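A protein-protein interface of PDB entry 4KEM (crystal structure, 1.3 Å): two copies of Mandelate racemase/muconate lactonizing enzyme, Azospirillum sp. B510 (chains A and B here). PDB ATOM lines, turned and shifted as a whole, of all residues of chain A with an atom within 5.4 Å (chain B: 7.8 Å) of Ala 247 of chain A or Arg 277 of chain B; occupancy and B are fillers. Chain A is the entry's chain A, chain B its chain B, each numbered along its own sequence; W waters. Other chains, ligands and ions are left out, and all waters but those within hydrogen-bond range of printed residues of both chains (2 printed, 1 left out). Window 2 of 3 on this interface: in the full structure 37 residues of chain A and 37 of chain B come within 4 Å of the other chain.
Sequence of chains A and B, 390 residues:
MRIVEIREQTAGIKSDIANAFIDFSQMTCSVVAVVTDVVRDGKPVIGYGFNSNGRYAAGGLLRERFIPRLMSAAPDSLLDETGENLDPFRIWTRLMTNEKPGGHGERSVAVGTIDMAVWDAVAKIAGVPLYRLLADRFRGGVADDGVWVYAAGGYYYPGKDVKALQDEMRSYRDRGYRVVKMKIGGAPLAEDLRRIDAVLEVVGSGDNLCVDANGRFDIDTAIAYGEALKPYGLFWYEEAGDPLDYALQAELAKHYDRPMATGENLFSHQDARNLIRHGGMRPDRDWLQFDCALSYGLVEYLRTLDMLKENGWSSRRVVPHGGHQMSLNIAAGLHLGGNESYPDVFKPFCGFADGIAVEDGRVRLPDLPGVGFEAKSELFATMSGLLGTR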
ATOM      1  N   ASP A 245      12.959  16.069 -20.128  1.00  0.00           N
ATOM      2  CA  ASP A 245      13.651  15.662 -21.361  1.00  0.00           C
ATOM      3  C   ASP A 245      14.995  15.038 -20.968  1.00  0.00           C
ATOM      4  O   ASP A 245      16.066  15.660 -21.013  1.00  0.00           O
ATOM      5  CB  ASP A 245      13.822  16.821 -22.326  1.00  0.00           C
ATOM      6  CG  ASP A 245      14.285  16.373 -23.672  1.00  0.00           C
ATOM      7  OD1 ASP A 245      14.759  15.217 -23.830  1.00  0.00           O
ATOM      8  OD2 ASP A 245      14.205  17.203 -24.618  1.00  0.00           O
ATOM      9  N   TYR A 246      14.929  13.802 -20.499  1.00  0.00           N
ATOM     10  CA  TYR A 246      16.102  13.144 -19.953  1.00  0.00           C
ATOM     11  C   TYR A 246      17.207  12.979 -21.003  1.00  0.00           C
ATOM     12  O   TYR A 246      18.391  13.187 -20.706  1.00  0.00           O
ATOM     13  CB  TYR A 246      15.705  11.817 -19.331  1.00  0.00           C
ATOM     14  CG  TYR A 246      14.608  11.933 -18.304  1.00  0.00           C
ATOM     15  CD1 TYR A 246      14.750  12.763 -17.200  1.00  0.00           C
ATOM     16  CD2 TYR A 246      13.443  11.197 -18.418  1.00  0.00           C
ATOM     17  CE1 TYR A 246      13.751  12.872 -16.249  1.00  0.00           C
ATOM     18  CE2 TYR A 246      12.448  11.287 -17.465  1.00  0.00           C
ATOM     19  CZ  TYR A 246      12.606  12.105 -16.373  1.00  0.00           C
ATOM     20  OH  TYR A 246      11.608  12.202 -15.438  1.00  0.00           O
ATOM     21  N   ALA A 247      16.829  12.616 -22.221  1.00  0.00           N
ATOM     22  CA  ALA A 247      17.802  12.485 -23.300  1.00  0.00           C
ATOM     23  C   ALA A 247      18.576  13.776 -23.576  1.00  0.00           C
ATOM     24  O   ALA A 247      19.746  13.728 -23.913  1.00  0.00           O
ATOM     25  CB  ALA A 247      17.115  12.000 -24.576  1.00  0.00           C
ATOM     26  N   LEU A 248      17.932  14.926 -23.423  1.00  0.00           N
ATOM     27  CA  LEU A 248      18.611  16.214 -23.626  1.00  0.00           C
ATOM     28  C   LEU A 248      19.725  16.410 -22.587  1.00  0.00           C
ATOM     29  O   LEU A 248      20.847  16.758 -22.930  1.00  0.00           O
ATOM     30  CB  LEU A 248      17.594  17.352 -23.565  1.00  0.00           C
ATOM     31  CG  LEU A 248      18.095  18.767 -23.857  1.00  0.00           C
ATOM     32  CD1 LEU A 248      16.920  19.681 -24.182  1.00  0.00           C
ATOM     33  CD2 LEU A 248      18.877  19.336 -22.681  1.00  0.00           C
ATOM     34  N   GLN A 249      19.413  16.173 -21.316  1.00  0.00           N
ATOM     35  CA  GLN A 249      20.431  16.286 -20.282  1.00  0.00           C
ATOM     36  C   GLN A 249      21.588  15.306 -20.531  1.00  0.00           C
ATOM     37  O   GLN A 249      22.753  15.648 -20.318  1.00  0.00           O
ATOM     38  CB  GLN A 249      19.791  16.054 -18.911  1.00  0.00           C
ATOM     39  CG  GLN A 249      20.760  16.121 -17.751  1.00  0.00           C
ATOM     40  CD  GLN A 249      21.436  17.478 -17.597  1.00  0.00           C
ATOM     41  OE1 GLN A 249      20.855  18.529 -17.905  1.00  0.00           O
ATOM     42  NE2 GLN A 249      22.666  17.459 -17.103  1.00  0.00           N
ATOM     43  N   ALA A 250      21.271  14.088 -20.962  1.00  0.00           N
ATOM     44  CA  ALA A 250      22.296  13.089 -21.261  1.00  0.00           C
ATOM     45  C   ALA A 250      23.217  13.560 -22.390  1.00  0.00           C
ATOM     46  O   ALA A 250      24.436  13.373 -22.333  1.00  0.00           O
ATOM     47  CB  ALA A 250      21.657  11.759 -21.625  1.00  0.00           C
ATOM     48  N   GLU A 251      22.641  14.177 -23.411  1.00  0.00           N
ATOM     49  CA  GLU A 251      23.433  14.698 -24.505  1.00  0.00           C
ATOM     50  C   GLU A 251      24.268  15.887 -24.037  1.00  0.00           C
ATOM     51  O   GLU A 251      25.430  15.994 -24.394  1.00  0.00           O
ATOM     52  CB  GLU A 251      22.535  15.097 -25.675  1.00  0.00           C
ATOM     53  CG  GLU A 251      23.294  15.733 -26.843  1.00  0.00           C
ATOM     54  CD  GLU A 251      24.199  14.756 -27.574  1.00  0.00           C
ATOM     55  OE1 GLU A 251      23.952  13.533 -27.518  1.00  0.00           O
ATOM     56  OE2 GLU A 251      25.163  15.216 -28.220  1.00  0.00           O
ATOM     57  N   LEU A 252      23.664  16.772 -23.241  1.00  0.00           N
ATOM     58  CA  LEU A 252      24.372  17.950 -22.726  1.00  0.00           C
ATOM     59  C   LEU A 252      25.614  17.539 -21.918  1.00  0.00           C
ATOM     60  O   LEU A 252      26.675  18.165 -22.017  1.00  0.00           O
ATOM     61  CB  LEU A 252      23.413  18.827 -21.905  1.00  0.00           C
ATOM     62  CG  LEU A 252      24.005  20.068 -21.231  1.00  0.00           C
ATOM     63  CD1 LEU A 252      24.633  21.007 -22.273  1.00  0.00           C
ATOM     64  CD2 LEU A 252      22.921  20.791 -20.437  1.00  0.00           C
ATOM     65  N   HIS A 278      17.829   7.604 -17.042  1.00  0.00           N
ATOM     66  CA  HIS A 278      17.851   8.048 -18.442  1.00  0.00           C
ATOM     67  C   HIS A 278      18.458   9.430 -18.703  1.00  0.00           C
ATOM     68  O   HIS A 278      18.616   9.821 -19.860  1.00  0.00           O
ATOM     69  CB  HIS A 278      16.422   8.021 -19.030  1.00  0.00           C
ATOM     70  CG  HIS A 278      15.704   6.723 -18.822  1.00  0.00           C
ATOM     71  ND1 HIS A 278      16.151   5.540 -19.360  1.00  0.00           N
ATOM     72  CD2 HIS A 278      14.579   6.420 -18.125  1.00  0.00           C
ATOM     73  CE1 HIS A 278      15.331   4.559 -19.004  1.00  0.00           C
ATOM     74  NE2 HIS A 278      14.370   5.069 -18.259  1.00  0.00           N
ATOM     75  N   GLY A 279      18.794  10.171 -17.647  1.00  0.00           N
ATOM     76  CA  GLY A 279      19.240  11.543 -17.787  1.00  0.00           C
ATOM     77  C   GLY A 279      20.738  11.774 -17.874  1.00  0.00           C
ATOM     78  O   GLY A 279      21.164  12.911 -18.046  1.00  0.00           O
ATOM     79  N   TYR B 246       9.118   3.115 -17.290  1.00  0.00           N
ATOM     80  CA  TYR B 246       9.397   2.756 -18.674  1.00  0.00           C
ATOM     81  C   TYR B 246      10.278   1.506 -18.758  1.00  0.00           C
ATOM     82  O   TYR B 246      10.041   0.619 -19.575  1.00  0.00           O
ATOM     83  CB  TYR B 246      10.036   3.950 -19.384  1.00  0.00           C
ATOM     84  CG  TYR B 246       9.203   5.213 -19.310  1.00  0.00           C
ATOM     85  CD1 TYR B 246       7.859   5.213 -19.694  1.00  0.00           C
ATOM     86  CD2 TYR B 246       9.759   6.402 -18.859  1.00  0.00           C
ATOM     87  CE1 TYR B 246       7.088   6.350 -19.608  1.00  0.00           C
ATOM     88  CE2 TYR B 246       9.004   7.555 -18.786  1.00  0.00           C
ATOM     89  CZ  TYR B 246       7.680   7.542 -19.198  1.00  0.00           C
ATOM     90  OH  TYR B 246       6.931   8.706 -19.112  1.00  0.00           O
ATOM     91  N   ALA B 250       9.731  -2.133 -20.796  1.00  0.00           N
ATOM     92  CA  ALA B 250      10.760  -2.654 -21.696  1.00  0.00           C
ATOM     93  C   ALA B 250      11.193  -4.069 -21.287  1.00  0.00           C
ATOM     94  O   ALA B 250      11.406  -4.911 -22.152  1.00  0.00           O
ATOM     95  CB  ALA B 250      11.971  -1.701 -21.749  1.00  0.00           C
ATOM     96  N   GLN B 270       5.889  15.430 -23.569  1.00  0.00           N
ATOM     97  CA  GLN B 270       7.178  15.090 -22.961  1.00  0.00           C
ATOM     98  C   GLN B 270       7.123  13.691 -22.346  1.00  0.00           C
ATOM     99  O   GLN B 270       8.052  12.879 -22.531  1.00  0.00           O
ATOM    100  CB  GLN B 270       7.595  16.083 -21.869  1.00  0.00           C
ATOM    101  CG  GLN B 270       7.937  17.479 -22.394  1.00  0.00           C
ATOM    102  CD  GLN B 270       6.761  18.460 -22.327  1.00  0.00           C
ATOM    103  OE1 GLN B 270       5.588  18.079 -22.451  1.00  0.00           O
ATOM    104  NE2 GLN B 270       7.084  19.737 -22.212  1.00  0.00           N
ATOM    105  N   ASP B 271       6.051  13.419 -21.605  1.00  0.00           N
ATOM    106  CA  ASP B 271       5.887  12.112 -20.972  1.00  0.00           C
ATOM    107  C   ASP B 271       5.643  11.028 -22.044  1.00  0.00           C
ATOM    108  O   ASP B 271       6.189   9.935 -21.952  1.00  0.00           O
ATOM    109  CB  ASP B 271       4.740  12.136 -19.955  1.00  0.00           C
ATOM    110  CG  ASP B 271       5.052  12.978 -18.728  1.00  0.00           C
ATOM    111  OD1 ASP B 271       6.063  12.705 -18.030  1.00  0.00           O
ATOM    112  OD2 ASP B 271       4.284  13.934 -18.461  1.00  0.00           O
ATOM    113  N   ALA B 272       4.848  11.332 -23.074  1.00  0.00           N
ATOM    114  CA  ALA B 272       4.650  10.411 -24.180  1.00  0.00           C
ATOM    115  C   ALA B 272       5.977  10.114 -24.875  1.00  0.00           C
ATOM    116  O   ALA B 272       6.251   8.965 -25.213  1.00  0.00           O
ATOM    117  CB  ALA B 272       3.609  10.956 -25.159  1.00  0.00           C
ATOM    118  N   ARG B 273       6.809  11.135 -25.100  1.00  0.00           N
ATOM    119  CA  ARG B 273       8.094  10.944 -25.749  1.00  0.00           C
ATOM    120  C   ARG B 273       9.008  10.055 -24.914  1.00  0.00           C
ATOM    121  O   ARG B 273       9.759   9.247 -25.452  1.00  0.00           O
ATOM    122  CB  ARG B 273       8.758  12.304 -25.993  1.00  0.00           C
ATOM    123  CG  ARG B 273      10.091  12.277 -26.725  1.00  0.00           C
ATOM    124  CD  ARG B 273      10.561  13.698 -27.067  1.00  0.00           C
ATOM    125  NE  ARG B 273      10.726  14.445 -25.829  1.00  0.00           N
ATOM    126  CZ  ARG B 273      10.647  15.765 -25.710  1.00  0.00           C
ATOM    127  NH1 ARG B 273      10.438  16.539 -26.766  1.00  0.00           N
ATOM    128  NH2 ARG B 273      10.791  16.311 -24.511  1.00  0.00           N
ATOM    129  N   ASN B 274       8.986  10.222 -23.599  1.00  0.00           N
ATOM    130  CA  ASN B 274       9.769   9.325 -22.749  1.00  0.00           C
ATOM    131  C   ASN B 274       9.322   7.867 -22.835  1.00  0.00           C
ATOM    132  O   ASN B 274      10.168   6.971 -22.816  1.00  0.00           O
ATOM    133  CB  ASN B 274       9.787   9.783 -21.291  1.00  0.00           C
ATOM    134  CG  ASN B 274      10.605  11.031 -21.083  1.00  0.00           C
ATOM    135  OD1 ASN B 274      11.535  11.318 -21.833  1.00  0.00           O
ATOM    136  ND2 ASN B 274      10.260  11.784 -20.043  1.00  0.00           N
ATOM    137  N   LEU B 275       8.025   7.629 -22.989  1.00  0.00           N
ATOM    138  CA  LEU B 275       7.539   6.268 -23.229  1.00  0.00           C
ATOM    139  C   LEU B 275       8.110   5.706 -24.528  1.00  0.00           C
ATOM    140  O   LEU B 275       8.604   4.568 -24.592  1.00  0.00           O
ATOM    141  CB  LEU B 275       6.023   6.252 -23.266  1.00  0.00           C
ATOM    142  CG  LEU B 275       5.404   4.900 -23.652  1.00  0.00           C
ATOM    143  CD1 LEU B 275       5.633   3.856 -22.590  1.00  0.00           C
ATOM    144  CD2 LEU B 275       3.936   5.044 -23.925  1.00  0.00           C
ATOM    145  N   ILE B 276       8.069   6.528 -25.565  1.00  0.00           N
ATOM    146  CA  ILE B 276       8.581   6.115 -26.878  1.00  0.00           C
ATOM    147  C   ILE B 276      10.089   5.849 -26.860  1.00  0.00           C
ATOM    148  O   ILE B 276      10.588   4.940 -27.518  1.00  0.00           O
ATOM    149  CB  ILE B 276       8.224   7.155 -27.971  1.00  0.00           C
ATOM    150  CG1 ILE B 276       6.699   7.299 -28.088  1.00  0.00           C
ATOM    151  CG2 ILE B 276       8.852   6.775 -29.318  1.00  0.00           C
ATOM    152  CD1 ILE B 276       5.964   6.015 -28.401  1.00  0.00           C
ATOM    153  N   ARG B 277      10.840   6.658 -26.116  1.00  0.00           N
ATOM    154  CA  ARG B 277      12.285   6.504 -26.056  1.00  0.00           C
ATOM    155  C   ARG B 277      12.722   5.351 -25.201  1.00  0.00           C
ATOM    156  O   ARG B 277      13.693   4.673 -25.539  1.00  0.00           O
ATOM    157  CB  ARG B 277      12.957   7.768 -25.514  1.00  0.00           C
ATOM    158  CG  ARG B 277      12.828   8.962 -26.435  1.00  0.00           C
ATOM    159  CD  ARG B 277      13.395  10.181 -25.782  1.00  0.00           C
ATOM    160  NE  ARG B 277      13.600  11.276 -26.727  1.00  0.00           N
ATOM    161  CZ  ARG B 277      13.842  12.528 -26.346  1.00  0.00           C
ATOM    162  NH1 ARG B 277      13.849  12.817 -25.058  1.00  0.00           N
ATOM    163  NH2 ARG B 277      14.035  13.494 -27.233  1.00  0.00           N
ATOM    164  N   HIS B 278      12.033   5.150 -24.074  1.00  0.00           N
ATOM    165  CA  HIS B 278      12.578   4.341 -22.971  1.00  0.00           C
ATOM    166  C   HIS B 278      11.713   3.137 -22.578  1.00  0.00           C
ATOM    167  O   HIS B 278      12.145   2.289 -21.793  1.00  0.00           O
ATOM    168  CB  HIS B 278      12.840   5.221 -21.728  1.00  0.00           C
ATOM    169  CG  HIS B 278      13.680   6.434 -22.007  1.00  0.00           C
ATOM    170  ND1 HIS B 278      14.961   6.355 -22.498  1.00  0.00           N
ATOM    171  CD2 HIS B 278      13.401   7.755 -21.891  1.00  0.00           C
ATOM    172  CE1 HIS B 278      15.441   7.576 -22.672  1.00  0.00           C
ATOM    173  NE2 HIS B 278      14.526   8.442 -22.288  1.00  0.00           N
ATOM    174  N   GLY B 279      10.506   3.039 -23.120  1.00  0.00           N
ATOM    175  CA  GLY B 279       9.563   2.005 -22.702  1.00  0.00           C
ATOM    176  C   GLY B 279       9.516   0.691 -23.470  1.00  0.00           C
ATOM    177  O   GLY B 279       8.729  -0.199 -23.117  1.00  0.00           O
ATOM    178  N   GLY B 280      10.346   0.545 -24.498  1.00  0.00           N
ATOM    179  CA  GLY B 280      10.353  -0.654 -25.320  1.00  0.00           C
ATOM    180  C   GLY B 280       9.019  -0.994 -25.978  1.00  0.00           C
ATOM    181  O   GLY B 280       8.688  -2.176 -26.165  1.00  0.00           O
ATOM    182  N   MET B 281       8.234   0.023 -26.301  1.00  0.00           N
ATOM    183  CA  MET B 281       7.016  -0.180 -27.070  1.00  0.00           C
ATOM    184  C   MET B 281       7.401  -0.455 -28.526  1.00  0.00           C
ATOM    185  O   MET B 281       8.395   0.053 -29.049  1.00  0.00           O
ATOM    186  CB  MET B 281       6.081   1.028 -26.959  1.00  0.00           C
ATOM    187  CG  MET B 281       5.671   1.363 -25.515  1.00  0.00           C
ATOM    188  SD  MET B 281       4.462   0.168 -24.883  1.00  0.00           S
ATOM    189  CE  MET B 281       3.018   0.648 -25.824  1.00  0.00           C
ATOM    190  N   MET B 307       5.548  14.199 -32.613  1.00  0.00           N
ATOM    191  CA  MET B 307       6.613  13.427 -32.001  1.00  0.00           C
ATOM    192  C   MET B 307       6.551  11.957 -32.412  1.00  0.00           C
ATOM    193  O   MET B 307       7.577  11.359 -32.758  1.00  0.00           O
ATOM    194  CB  MET B 307       6.542  13.602 -30.474  1.00  0.00           C
ATOM    195  CG  MET B 307       7.582  12.834 -29.680  1.00  0.00           C
ATOM    196  SD  MET B 307       7.175  11.105 -29.391  1.00  0.00           S
ATOM    197  CE  MET B 307       5.678  11.289 -28.415  1.00  0.00           C
ATOM    198  N   ASN B 311       9.426   9.802 -34.499  1.00  0.00           N
ATOM    199  CA  ASN B 311      10.009   8.619 -33.880  1.00  0.00           C
ATOM    200  C   ASN B 311       9.528   7.299 -34.474  1.00  0.00           C
ATOM    201  O   ASN B 311       9.621   6.255 -33.821  1.00  0.00           O
ATOM    202  CB  ASN B 311       9.749   8.638 -32.368  1.00  0.00           C
ATOM    203  CG  ASN B 311      10.584   9.678 -31.643  1.00  0.00           C
ATOM    204  OD1 ASN B 311      11.680   9.384 -31.156  1.00  0.00           O
ATOM    205  ND2 ASN B 311      10.074  10.896 -31.560  1.00  0.00           N
ATOM    206  N   TRP B 313       6.499   6.119 -35.397  1.00  0.00           N
ATOM    207  CA  TRP B 313       5.218   5.544 -35.016  1.00  0.00           C
ATOM    208  C   TRP B 313       4.090   6.113 -35.875  1.00  0.00           C
ATOM    209  O   TRP B 313       4.043   7.314 -36.114  1.00  0.00           O
ATOM    210  CB  TRP B 313       4.907   5.857 -33.562  1.00  0.00           C
ATOM    211  CG  TRP B 313       5.573   4.946 -32.603  1.00  0.00           C
ATOM    212  CD1 TRP B 313       6.882   4.973 -32.211  1.00  0.00           C
ATOM    213  CD2 TRP B 313       4.958   3.868 -31.895  1.00  0.00           C
ATOM    214  NE1 TRP B 313       7.123   3.953 -31.311  1.00  0.00           N
ATOM    215  CE2 TRP B 313       5.949   3.273 -31.095  1.00  0.00           C
ATOM    216  CE3 TRP B 313       3.660   3.344 -31.860  1.00  0.00           C
ATOM    217  CZ2 TRP B 313       5.678   2.193 -30.272  1.00  0.00           C
ATOM    218  CZ3 TRP B 313       3.404   2.280 -31.044  1.00  0.00           C
ATOM    219  CH2 TRP B 313       4.400   1.713 -30.264  1.00  0.00           C
HETATM  220  O   HOH W   1      14.545  16.287 -27.094  1.00  0.00           O
HETATM  221  O   HOH W   2      12.314   3.894 -16.586  1.00  0.00           O
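Printed residues of chain B within 4 Å of Ala 247 of chain A: Arg 277 (3.4 Å). Arg 277 of chain B touches two residues of chain A. Printed residues of chain B within 4 Å of Tyr 246 of chain A: Asn 274 (3.4 Å). Of the printed residues of chain A, Asn 274 of chain B touches Tyr 246 (3.4 Å). Of the printed residues of chain A, Arg 273 of chain B touches Asp 245 (3.5 Å). Of the printed residues of chain B, Asp 245 of chain A touches Arg 273 and Arg 277. Printed residues of chain A within 4 Å of His 278 of chain B: His 278. Ala 272 of chain B touches none of the printed residues of chain A. The nearest residue of chain A that does not touch Arg 277 of chain B is Tyr 246 of chain A (4.8 Å).
ND1 of His 278 of chain A lies within hydrogen-bond range of ND1 of His 278 of chain B (3.5 Å). The guanidinium group (NH1) of Arg 277 of chain B lies within salt-bridge range of the side-chain carboxylate (OD1) of Asp 245 of chain A. The guanidinium group (NH2) of Arg 273 of chain B is in salt-bridge range of the side-chain carboxylate (OD2) of Asp 245 of chain A (3.5 Å).
Water W1 lies within hydrogen-bond range of the side-chain carboxylate of Asp 245 of chain A (2.7 Å) and the guanidinium group of Arg 277 of chain B (2.8 Å). Water W2 bridges a ring nitrogen (NE2) of His 278 of chain A (2.9 Å) and the backbone NH (N) of Tyr 246 of chain B (3.4 Å).
Of the 10 printed residues of chain A, 4 touch a printed residue of chain B. Printed residues of chain A that touch a printed residue of chain B: Asp 245, Tyr 246, Ala 247 and His 278. Among the printed residues, 5 pairs touch across the chains.
His 278 of chain B touches its own counterpart, His 278 of chain A. Positions printed for both chains: 246, 250, 278 and 279. Of the 5 pairs that touch across the chains among the printed residues, 1 has its exchanged pair printed and touching as well.
N of Leu 248 of chain A is in hydrogen-bond range of OD1 of Asp 245 of chain A (3.2 Å).
Tyr 246 of chain A touches Asn 274 of chain B. Ala 247 of chain A touches Arg 277 of chain B.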
